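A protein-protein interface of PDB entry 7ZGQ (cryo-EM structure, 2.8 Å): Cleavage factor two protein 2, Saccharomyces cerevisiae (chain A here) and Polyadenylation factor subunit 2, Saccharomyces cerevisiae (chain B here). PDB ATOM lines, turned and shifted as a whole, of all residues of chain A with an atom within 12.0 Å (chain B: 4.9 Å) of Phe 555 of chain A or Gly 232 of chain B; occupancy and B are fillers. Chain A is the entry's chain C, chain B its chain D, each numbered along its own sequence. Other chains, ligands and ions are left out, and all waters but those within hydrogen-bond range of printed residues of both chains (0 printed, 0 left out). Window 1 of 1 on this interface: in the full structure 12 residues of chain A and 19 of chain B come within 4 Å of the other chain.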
ATOM      1  N   ILE A 544      13.597  13.434  22.018  1.00  0.00           N
ATOM      2  CA  ILE A 544      14.982  13.876  21.920  1.00  0.00           C
ATOM      3  C   ILE A 544      15.622  13.178  20.729  1.00  0.00           C
ATOM      4  O   ILE A 544      15.884  11.971  20.775  1.00  0.00           O
ATOM      5  CB  ILE A 544      15.755  13.581  23.213  1.00  0.00           C
ATOM      6  CG1 ILE A 544      15.028  14.183  24.417  1.00  0.00           C
ATOM      7  CG2 ILE A 544      17.170  14.124  23.124  1.00  0.00           C
ATOM      8  CD1 ILE A 544      14.839  15.680  24.329  1.00  0.00           C
ATOM      9  N   LYS A 545      15.874  13.934  19.665  1.00  0.00           N
ATOM     10  CA  LYS A 545      16.491  13.369  18.473  1.00  0.00           C
ATOM     11  C   LYS A 545      17.931  12.981  18.782  1.00  0.00           C
ATOM     12  O   LYS A 545      18.715  13.807  19.261  1.00  0.00           O
ATOM     13  CB  LYS A 545      16.436  14.370  17.322  1.00  0.00           C
ATOM     14  N   LYS A 546      18.277  11.724  18.515  1.00  0.00           N
ATOM     15  CA  LYS A 546      19.596  11.191  18.835  1.00  0.00           C
ATOM     16  C   LYS A 546      20.115  10.432  17.622  1.00  0.00           C
ATOM     17  O   LYS A 546      19.502   9.453  17.186  1.00  0.00           O
ATOM     18  CB  LYS A 546      19.539  10.293  20.073  1.00  0.00           C
ATOM     19  CG  LYS A 546      20.529   9.139  20.080  1.00  0.00           C
ATOM     20  CD  LYS A 546      20.827   8.664  21.497  1.00  0.00           C
ATOM     21  CE  LYS A 546      19.595   8.731  22.387  1.00  0.00           C
ATOM     22  NZ  LYS A 546      18.603   7.676  22.042  1.00  0.00           N
ATOM     23  N   ASP A 547      21.225  10.902  17.064  1.00  0.00           N
ATOM     24  CA  ASP A 547      21.890  10.258  15.945  1.00  0.00           C
ATOM     25  C   ASP A 547      23.053   9.408  16.457  1.00  0.00           C
ATOM     26  O   ASP A 547      23.200   9.172  17.660  1.00  0.00           O
ATOM     27  CB  ASP A 547      22.343  11.309  14.930  1.00  0.00           C
ATOM     28  CG  ASP A 547      23.314  12.308  15.520  1.00  0.00           C
ATOM     29  OD1 ASP A 547      22.941  13.003  16.486  1.00  0.00           O
ATOM     30  OD2 ASP A 547      24.451  12.403  15.015  1.00  0.00           O
ATOM     31  N   ASP A 548      23.888   8.932  15.528  1.00  0.00           N
ATOM     32  CA  ASP A 548      25.025   8.097  15.905  1.00  0.00           C
ATOM     33  C   ASP A 548      26.004   8.855  16.791  1.00  0.00           C
ATOM     34  O   ASP A 548      26.537   8.298  17.758  1.00  0.00           O
ATOM     35  CB  ASP A 548      25.731   7.579  14.652  1.00  0.00           C
ATOM     36  CG  ASP A 548      24.808   6.790  13.750  1.00  0.00           C
ATOM     37  OD1 ASP A 548      23.579   6.842  13.967  1.00  0.00           O
ATOM     38  OD2 ASP A 548      25.309   6.116  12.826  1.00  0.00           O
ATOM     39  N   TYR A 549      26.256  10.127  16.478  1.00  0.00           N
ATOM     40  CA  TYR A 549      27.186  10.932  17.260  1.00  0.00           C
ATOM     41  C   TYR A 549      26.663  11.257  18.652  1.00  0.00           C
ATOM     42  O   TYR A 549      27.434  11.749  19.483  1.00  0.00           O
ATOM     43  CB  TYR A 549      27.505  12.229  16.518  1.00  0.00           C
ATOM     44  CG  TYR A 549      28.123  12.019  15.155  1.00  0.00           C
ATOM     45  CD1 TYR A 549      27.328  11.873  14.028  1.00  0.00           C
ATOM     46  CD2 TYR A 549      29.500  11.968  14.997  1.00  0.00           C
ATOM     47  CE1 TYR A 549      27.883  11.681  12.782  1.00  0.00           C
ATOM     48  CE2 TYR A 549      30.067  11.778  13.751  1.00  0.00           C
ATOM     49  CZ  TYR A 549      29.253  11.634  12.649  1.00  0.00           C
ATOM     50  OH  TYR A 549      29.807  11.444  11.406  1.00  0.00           O
ATOM     51  N   GLY A 550      25.387  11.001  18.923  1.00  0.00           N
ATOM     52  CA  GLY A 550      24.790  11.347  20.196  1.00  0.00           C
ATOM     53  C   GLY A 550      23.426  11.976  20.012  1.00  0.00           C
ATOM     54  O   GLY A 550      22.750  11.711  19.015  1.00  0.00           O
ATOM     55  N   THR A 551      23.008  12.811  20.959  1.00  0.00           N
ATOM     56  CA  THR A 551      21.731  13.511  20.868  1.00  0.00           C
ATOM     57  C   THR A 551      21.989  14.924  20.362  1.00  0.00           C
ATOM     58  O   THR A 551      22.743  15.683  20.980  1.00  0.00           O
ATOM     59  CB  THR A 551      21.025  13.541  22.220  1.00  0.00           C
ATOM     60  OG1 THR A 551      21.674  14.487  23.076  1.00  0.00           O
ATOM     61  CG2 THR A 551      21.055  12.170  22.874  1.00  0.00           C
ATOM     62  N   VAL A 552      21.370  15.277  19.236  1.00  0.00           N
ATOM     63  CA  VAL A 552      21.499  16.637  18.724  1.00  0.00           C
ATOM     64  C   VAL A 552      20.733  17.580  19.640  1.00  0.00           C
ATOM     65  O   VAL A 552      19.517  17.447  19.825  1.00  0.00           O
ATOM     66  CB  VAL A 552      21.017  16.719  17.269  1.00  0.00           C
ATOM     67  CG1 VAL A 552      19.689  15.999  17.094  1.00  0.00           C
ATOM     68  CG2 VAL A 552      20.898  18.171  16.836  1.00  0.00           C
ATOM     69  N   VAL A 553      21.450  18.533  20.234  1.00  0.00           N
ATOM     70  CA  VAL A 553      20.883  19.469  21.193  1.00  0.00           C
ATOM     71  C   VAL A 553      21.202  20.887  20.737  1.00  0.00           C
ATOM     72  O   VAL A 553      21.917  21.104  19.759  1.00  0.00           O
ATOM     73  CB  VAL A 553      21.408  19.232  22.625  1.00  0.00           C
ATOM     74  CG1 VAL A 553      21.231  17.777  23.026  1.00  0.00           C
ATOM     75  CG2 VAL A 553      22.872  19.638  22.722  1.00  0.00           C
ATOM     76  N   ASP A 554      20.642  21.855  21.458  1.00  0.00           N
ATOM     77  CA  ASP A 554      20.972  23.252  21.214  1.00  0.00           C
ATOM     78  C   ASP A 554      22.448  23.459  21.522  1.00  0.00           C
ATOM     79  O   ASP A 554      22.929  23.070  22.590  1.00  0.00           O
ATOM     80  CB  ASP A 554      20.091  24.158  22.080  1.00  0.00           C
ATOM     81  CG  ASP A 554      20.682  25.553  22.302  1.00  0.00           C
ATOM     82  OD1 ASP A 554      21.517  26.021  21.499  1.00  0.00           O
ATOM     83  OD2 ASP A 554      20.245  26.220  23.263  1.00  0.00           O
ATOM     84  N   PHE A 555      23.165  24.069  20.587  1.00  0.00           N
ATOM     85  CA  PHE A 555      24.604  24.230  20.716  1.00  0.00           C
ATOM     86  C   PHE A 555      25.007  25.640  21.117  1.00  0.00           C
ATOM     87  O   PHE A 555      26.203  25.950  21.132  1.00  0.00           O
ATOM     88  CB  PHE A 555      25.280  23.827  19.405  1.00  0.00           C
ATOM     89  CG  PHE A 555      25.711  22.394  19.380  1.00  0.00           C
ATOM     90  CD1 PHE A 555      26.095  21.756  20.547  1.00  0.00           C
ATOM     91  CD2 PHE A 555      25.670  21.665  18.209  1.00  0.00           C
ATOM     92  CE1 PHE A 555      26.474  20.432  20.536  1.00  0.00           C
ATOM     93  CE2 PHE A 555      26.040  20.337  18.195  1.00  0.00           C
ATOM     94  CZ  PHE A 555      26.447  19.722  19.356  1.00  0.00           C
ATOM     95  N   THR A 556      24.041  26.497  21.442  1.00  0.00           N
ATOM     96  CA  THR A 556      24.331  27.826  21.961  1.00  0.00           C
ATOM     97  C   THR A 556      24.191  27.903  23.474  1.00  0.00           C
ATOM     98  O   THR A 556      24.699  28.850  24.086  1.00  0.00           O
ATOM     99  CB  THR A 556      23.413  28.864  21.311  1.00  0.00           C
ATOM    100  N   MET A 557      23.514  26.931  24.090  1.00  0.00           N
ATOM    101  CA  MET A 557      23.354  26.941  25.540  1.00  0.00           C
ATOM    102  C   MET A 557      24.651  26.619  26.269  1.00  0.00           C
ATOM    103  O   MET A 557      24.708  26.754  27.495  1.00  0.00           O
ATOM    104  CB  MET A 557      22.261  25.957  25.965  1.00  0.00           C
ATOM    105  CG  MET A 557      22.401  24.561  25.384  1.00  0.00           C
ATOM    106  SD  MET A 557      21.876  23.289  26.551  1.00  0.00           S
ATOM    107  CE  MET A 557      21.884  21.836  25.506  1.00  0.00           C
ATOM    108  N   PHE A 558      25.686  26.189  25.549  1.00  0.00           N
ATOM    109  CA  PHE A 558      26.997  25.963  26.141  1.00  0.00           C
ATOM    110  C   PHE A 558      27.880  27.202  26.115  1.00  0.00           C
ATOM    111  O   PHE A 558      29.088  27.083  26.343  1.00  0.00           O
ATOM    112  CB  PHE A 558      27.711  24.814  25.423  1.00  0.00           C
ATOM    113  CG  PHE A 558      26.879  23.575  25.292  1.00  0.00           C
ATOM    114  CD1 PHE A 558      26.525  22.843  26.411  1.00  0.00           C
ATOM    115  CD2 PHE A 558      26.446  23.147  24.051  1.00  0.00           C
ATOM    116  CE1 PHE A 558      25.759  21.705  26.290  1.00  0.00           C
ATOM    117  CE2 PHE A 558      25.682  22.009  23.926  1.00  0.00           C
ATOM    118  CZ  PHE A 558      25.338  21.290  25.045  1.00  0.00           C
ATOM    119  N   LEU A 559      27.315  28.372  25.835  1.00  0.00           N
ATOM    120  CA  LEU A 559      28.097  29.595  25.803  1.00  0.00           C
ATOM    121  C   LEU A 559      28.696  29.866  27.182  1.00  0.00           C
ATOM    122  O   LEU A 559      27.979  29.785  28.190  1.00  0.00           O
ATOM    123  CB  LEU A 559      27.227  30.774  25.365  1.00  0.00           C
ATOM    124  N   PRO A 560      29.993  30.178  27.271  1.00  0.00           N
ATOM    125  CA  PRO A 560      30.597  30.416  28.592  1.00  0.00           C
ATOM    126  C   PRO A 560      30.014  31.611  29.326  1.00  0.00           C
ATOM    127  O   PRO A 560      30.160  31.685  30.553  1.00  0.00           O
ATOM    128  CB  PRO A 560      32.080  30.632  28.266  1.00  0.00           C
ATOM    129  N   ASP A 561      29.370  32.537  28.619  1.00  0.00           N
ATOM    130  CA  ASP A 561      28.757  33.719  29.224  1.00  0.00           C
ATOM    131  C   ASP A 561      29.765  34.531  30.034  1.00  0.00           C
ATOM    132  O   ASP A 561      29.425  35.565  30.610  1.00  0.00           O
ATOM    133  CB  ASP A 561      27.573  33.319  30.109  1.00  0.00           C
ATOM    134  N   TRP B 227      34.253  12.626  25.158  1.00  0.00           N
ATOM    135  CA  TRP B 227      32.954  12.644  24.504  1.00  0.00           C
ATOM    136  C   TRP B 227      31.864  12.650  25.566  1.00  0.00           C
ATOM    137  O   TRP B 227      31.979  11.952  26.579  1.00  0.00           O
ATOM    138  CB  TRP B 227      32.794  11.434  23.580  1.00  0.00           C
ATOM    139  CG  TRP B 227      31.813  11.638  22.468  1.00  0.00           C
ATOM    140  CD1 TRP B 227      30.533  12.091  22.576  1.00  0.00           C
ATOM    141  CD2 TRP B 227      32.036  11.393  21.076  1.00  0.00           C
ATOM    142  NE1 TRP B 227      29.944  12.145  21.338  1.00  0.00           N
ATOM    143  CE2 TRP B 227      30.846  11.722  20.399  1.00  0.00           C
ATOM    144  CE3 TRP B 227      33.128  10.931  20.335  1.00  0.00           C
ATOM    145  CZ2 TRP B 227      30.716  11.602  19.019  1.00  0.00           C
ATOM    146  CZ3 TRP B 227      32.996  10.812  18.965  1.00  0.00           C
ATOM    147  CH2 TRP B 227      31.799  11.147  18.321  1.00  0.00           C
ATOM    148  N   GLU B 230      25.954  11.076  26.725  1.00  0.00           N
ATOM    149  CA  GLU B 230      24.659  10.968  26.065  1.00  0.00           C
ATOM    150  C   GLU B 230      24.551  11.853  24.834  1.00  0.00           C
ATOM    151  O   GLU B 230      24.049  11.413  23.795  1.00  0.00           O
ATOM    152  CB  GLU B 230      23.537  11.318  27.052  1.00  0.00           C
ATOM    153  CG  GLU B 230      23.096  10.161  27.932  1.00  0.00           C
ATOM    154  CD  GLU B 230      23.883  10.078  29.227  1.00  0.00           C
ATOM    155  OE1 GLU B 230      23.675  10.940  30.106  1.00  0.00           O
ATOM    156  OE2 GLU B 230      24.707   9.150  29.366  1.00  0.00           O
ATOM    157  N   MET B 231      25.017  13.092  24.924  1.00  0.00           N
ATOM    158  CA  MET B 231      24.871  14.063  23.854  1.00  0.00           C
ATOM    159  C   MET B 231      26.088  14.052  22.938  1.00  0.00           C
ATOM    160  O   MET B 231      27.145  13.514  23.271  1.00  0.00           O
ATOM    161  CB  MET B 231      24.669  15.460  24.438  1.00  0.00           C
ATOM    162  CG  MET B 231      23.560  15.537  25.473  1.00  0.00           C
ATOM    163  SD  MET B 231      23.575  17.075  26.411  1.00  0.00           S
ATOM    164  CE  MET B 231      24.816  17.993  25.512  1.00  0.00           C
ATOM    165  N   GLY B 232      25.923  14.659  21.767  1.00  0.00           N
ATOM    166  CA  GLY B 232      27.043  14.860  20.874  1.00  0.00           C
ATOM    167  C   GLY B 232      27.784  16.128  21.237  1.00  0.00           C
ATOM    168  O   GLY B 232      27.361  17.228  20.876  1.00  0.00           O
ATOM    169  N   LEU B 233      28.893  15.986  21.957  1.00  0.00           N
ATOM    170  CA  LEU B 233      29.621  17.143  22.469  1.00  0.00           C
ATOM    171  C   LEU B 233      31.033  16.704  22.812  1.00  0.00           C
ATOM    172  O   LEU B 233      31.215  15.771  23.600  1.00  0.00           O
ATOM    173  CB  LEU B 233      28.918  17.725  23.696  1.00  0.00           C
ATOM    174  CG  LEU B 233      29.513  18.989  24.311  1.00  0.00           C
ATOM    175  CD1 LEU B 233      29.160  20.203  23.474  1.00  0.00           C
ATOM    176  CD2 LEU B 233      29.023  19.161  25.737  1.00  0.00           C
ATOM    177  N   ILE B 234      32.023  17.371  22.226  1.00  0.00           N
ATOM    178  CA  ILE B 234      33.428  17.025  22.401  1.00  0.00           C
ATOM    179  C   ILE B 234      34.079  18.084  23.277  1.00  0.00           C
ATOM    180  O   ILE B 234      33.932  19.285  23.024  1.00  0.00           O
ATOM    181  CB  ILE B 234      34.154  16.912  21.049  1.00  0.00           C
ATOM    182  CG1 ILE B 234      33.358  16.030  20.087  1.00  0.00           C
ATOM    183  CG2 ILE B 234      35.557  16.364  21.242  1.00  0.00           C
ATOM    184  CD1 ILE B 234      33.258  14.591  20.523  1.00  0.00           C
ATOM    185  N   TRP B 246      33.427  21.271  21.348  1.00  0.00           N
ATOM    186  CA  TRP B 246      33.369  21.115  19.905  1.00  0.00           C
ATOM    187  C   TRP B 246      32.034  20.519  19.476  1.00  0.00           C
ATOM    188  O   TRP B 246      31.128  20.294  20.283  1.00  0.00           O
ATOM    189  CB  TRP B 246      34.525  20.245  19.411  1.00  0.00           C
ATOM    190  CG  TRP B 246      35.866  20.723  19.841  1.00  0.00           C
ATOM    191  CD1 TRP B 246      36.536  20.374  20.973  1.00  0.00           C
ATOM    192  CD2 TRP B 246      36.710  21.642  19.140  1.00  0.00           C
ATOM    193  NE1 TRP B 246      37.746  21.018  21.022  1.00  0.00           N
ATOM    194  CE2 TRP B 246      37.878  21.803  19.908  1.00  0.00           C
ATOM    195  CE3 TRP B 246      36.592  22.346  17.938  1.00  0.00           C
ATOM    196  CZ2 TRP B 246      38.919  22.636  19.513  1.00  0.00           C
ATOM    197  CZ3 TRP B 246      37.627  23.171  17.549  1.00  0.00           C
ATOM    198  CH2 TRP B 246      38.775  23.311  18.335  1.00  0.00           C
ATOM    199  N   ASP B 247      31.930  20.266  18.179  1.00  0.00           N
ATOM    200  CA  ASP B 247      30.724  19.722  17.560  1.00  0.00           C
ATOM    201  C   ASP B 247      31.075  18.453  16.801  1.00  0.00           C
ATOM    202  O   ASP B 247      31.834  18.516  15.816  1.00  0.00           O
ATOM    203  CB  ASP B 247      30.103  20.754  16.619  1.00  0.00           C
ATOM    204  CG  ASP B 247      28.660  20.449  16.286  1.00  0.00           C
ATOM    205  OD1 ASP B 247      28.285  19.258  16.263  1.00  0.00           O
ATOM    206  OD2 ASP B 247      27.896  21.407  16.052  1.00  0.00           O
ATOM    207  N   PRO B 248      30.564  17.287  17.206  1.00  0.00           N
ATOM    208  CA  PRO B 248      30.819  16.060  16.438  1.00  0.00           C
ATOM    209  C   PRO B 248      30.220  16.070  15.042  1.00  0.00           C
ATOM    210  O   PRO B 248      30.619  15.245  14.212  1.00  0.00           O
ATOM    211  CB  PRO B 248      30.174  14.964  17.302  1.00  0.00           C
ATOM    212  CG  PRO B 248      30.023  15.572  18.658  1.00  0.00           C
ATOM    213  CD  PRO B 248      29.780  17.025  18.421  1.00  0.00           C
ATOM    214  N   ARG B 249      29.279  16.969  14.754  1.00  0.00           N
ATOM    215  CA  ARG B 249      28.622  17.018  13.453  1.00  0.00           C
ATOM    216  C   ARG B 249      29.041  18.237  12.642  1.00  0.00           C
ATOM    217  O   ARG B 249      29.476  18.083  11.497  1.00  0.00           O
ATOM    218  CB  ARG B 249      27.100  16.984  13.639  1.00  0.00           C
ATOM    219  CG  ARG B 249      26.629  15.893  14.580  1.00  0.00           C
ATOM    220  CD  ARG B 249      25.127  15.936  14.779  1.00  0.00           C
ATOM    221  NE  ARG B 249      24.710  15.093  15.893  1.00  0.00           N
ATOM    222  CZ  ARG B 249      24.581  15.513  17.144  1.00  0.00           C
ATOM    223  NH1 ARG B 249      24.826  16.769  17.479  1.00  0.00           N
ATOM    224  NH2 ARG B 249      24.197  14.653  18.081  1.00  0.00           N
ATOM    225  N   ILE B 254      32.039  25.211  19.189  1.00  0.00           N
ATOM    226  CA  ILE B 254      30.802  25.850  19.620  1.00  0.00           C
ATOM    227  C   ILE B 254      31.004  26.726  20.847  1.00  0.00           C
ATOM    228  O   ILE B 254      30.246  27.684  21.044  1.00  0.00           O
ATOM    229  CB  ILE B 254      29.720  24.792  19.897  1.00  0.00           C
ATOM    230  CG1 ILE B 254      30.196  23.816  20.971  1.00  0.00           C
ATOM    231  CG2 ILE B 254      29.367  24.049  18.620  1.00  0.00           C
ATOM    232  CD1 ILE B 254      29.207  23.606  22.081  1.00  0.00           C
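The side-chain carboxylate (OD1) of Asp 547 of chain A lies within salt-bridge range of the guanidinium group (NH2) of Arg 249 of chain B (2.6 Å).
The indole nitrogen of Trp 227 of chain B lies within hydrogen-bond range of the backbone carbonyl oxygen of Tyr 549 of chain A.
O of Gly 550 of chain A sits close to NH2 of Arg 249 of chain B (3.4 Å).
The backbone NH of Thr 551 of chain A lies close to the backbone carbonyl oxygen of Glu 230 of chain B (3.3 Å).
The backbone carbonyl oxygen of Thr 551 of chain A is in hydrogen-bond range of the backbone NH of Gly 232 of chain B, at 3.4 Å.
O of Thr 551 of chain A sits close to NH2 of Arg 249 of chain B, 3.4 Å away.
The guanidinium group of Arg 249 of chain B lies close to the backbone NH of Val 552 of chain A.
Of the 18 printed residues of chain A, 8 touch a printed residue of chain B.
Hydrophobic or aromatic side chains of chain A that line the printed part of chain B: Tyr 549, Val 552, Val 553, Phe 555 and Phe 558.
Of the 11 printed residues of chain B, 9 touch a printed residue of chain A.
Printed residues of chain B that touch a printed residue of chain A: Trp 227, Glu 230, Met 231, Gly 232, Leu 233, Asp 247, Pro 248, Arg 249 and Ile 254.
Hydrophobic or aromatic side chains of chain B within 4 Å of the printed part of chain A: Trp 227, Met 231, Leu 233, Pro 248 and Ile 254.
Along chain B the printed residues that touch a printed residue of chain A span positions 227 to 254.
Among the printed residues, Asp or Glu carboxylates within 4 Å of a Lys or Arg side-chain nitrogen of the other chain: Asp 547 of chain A with Arg 249 of chain B (2.6 Å).
Of the printed residues of chain B, Phe 555 of chain A touches Gly 232, Leu 233, Asp 247, Arg 249 and Ile 254.
No residue of chain A comes within 4 Å of Ile 234 of chain B.
Asp 247 of chain B touches one residue of chain A.
Of chain A, only Tyr 549 comes within 4 Å of Pro 248 of chain B.
Printed residues of chain A within 4 Å of Ile 254 of chain B: Phe 555 and Phe 558.
Printed residues of chain B within 4 Å of Thr 551 of chain A: Glu 230 (3.2 Å), Met 231 (3.2 Å), Gly 232 (3.4 Å) and Arg 249 (3.2 Å).
Printed residues of chain B within 4 Å of Val 552 of chain A: Arg 249.
Printed residues of chain B within 4 Å of Phe 558 of chain A: Met 231 (3.4 Å), Leu 233 (3.9 Å) and Ile 254 (3.4 Å).
Of the printed residues of chain A, Glu 230 of chain B touches Gly 550 (3.7 Å) and Thr 551 (3.2 Å).
Of the printed residues of chain B, Gly 550 of chain A touches Glu 230 (3.7 Å), Gly 232 (3.8 Å) and Arg 249 (3.4 Å).
Lys 545 of chain A touches none of the printed residues of chain B.
The nearest printed residue of chain B that does not touch Val 553 of chain A is Arg 249 of chain B (4.7 Å).
Tyr 549 of chain A touches Pro 248 of chain B.
CA of Gly 550 of chain A touches O of Glu 230 of chain B, at 3.7 Å.
Met 231 of chain B touches Thr 551 of chain A.
Val 553 of chain A touches Met 231 of chain B (CG2 to CE, 3.8 Å).
CD1 of Leu 233 of chain B touches CE1 of Phe 555 of chain A (3.99 Å).
Arg 249 of chain B touches Phe 555 of chain A (NH1 to CE2, 3.8 Å).
O of Phe 555 of chain A touches CB of Ile 254 of chain B (3.9 Å).
Phe 558 of chain A touches Met 231 of chain B (CZ to CE, 3.4 Å).
Leu 233 of chain B touches Phe 558 of chain A.
Phe 558 of chain A touches Ile 254 of chain B.
The backbone carbonyl oxygen (O) of Lys 545 of chain A sits at hydrogen-bond distance from the backbone NH (N) of Val 552 of chain A (3.0 Å).
The side-chain carboxylate (OD2) of Asp 547 of chain A sits close to the backbone NH (N) of Tyr 549 of chain A (3.3 Å).
The backbone NH of Arg 249 of chain B sits at hydrogen-bond distance from the side-chain carboxylate of Asp 247 of chain B (2.9 Å).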
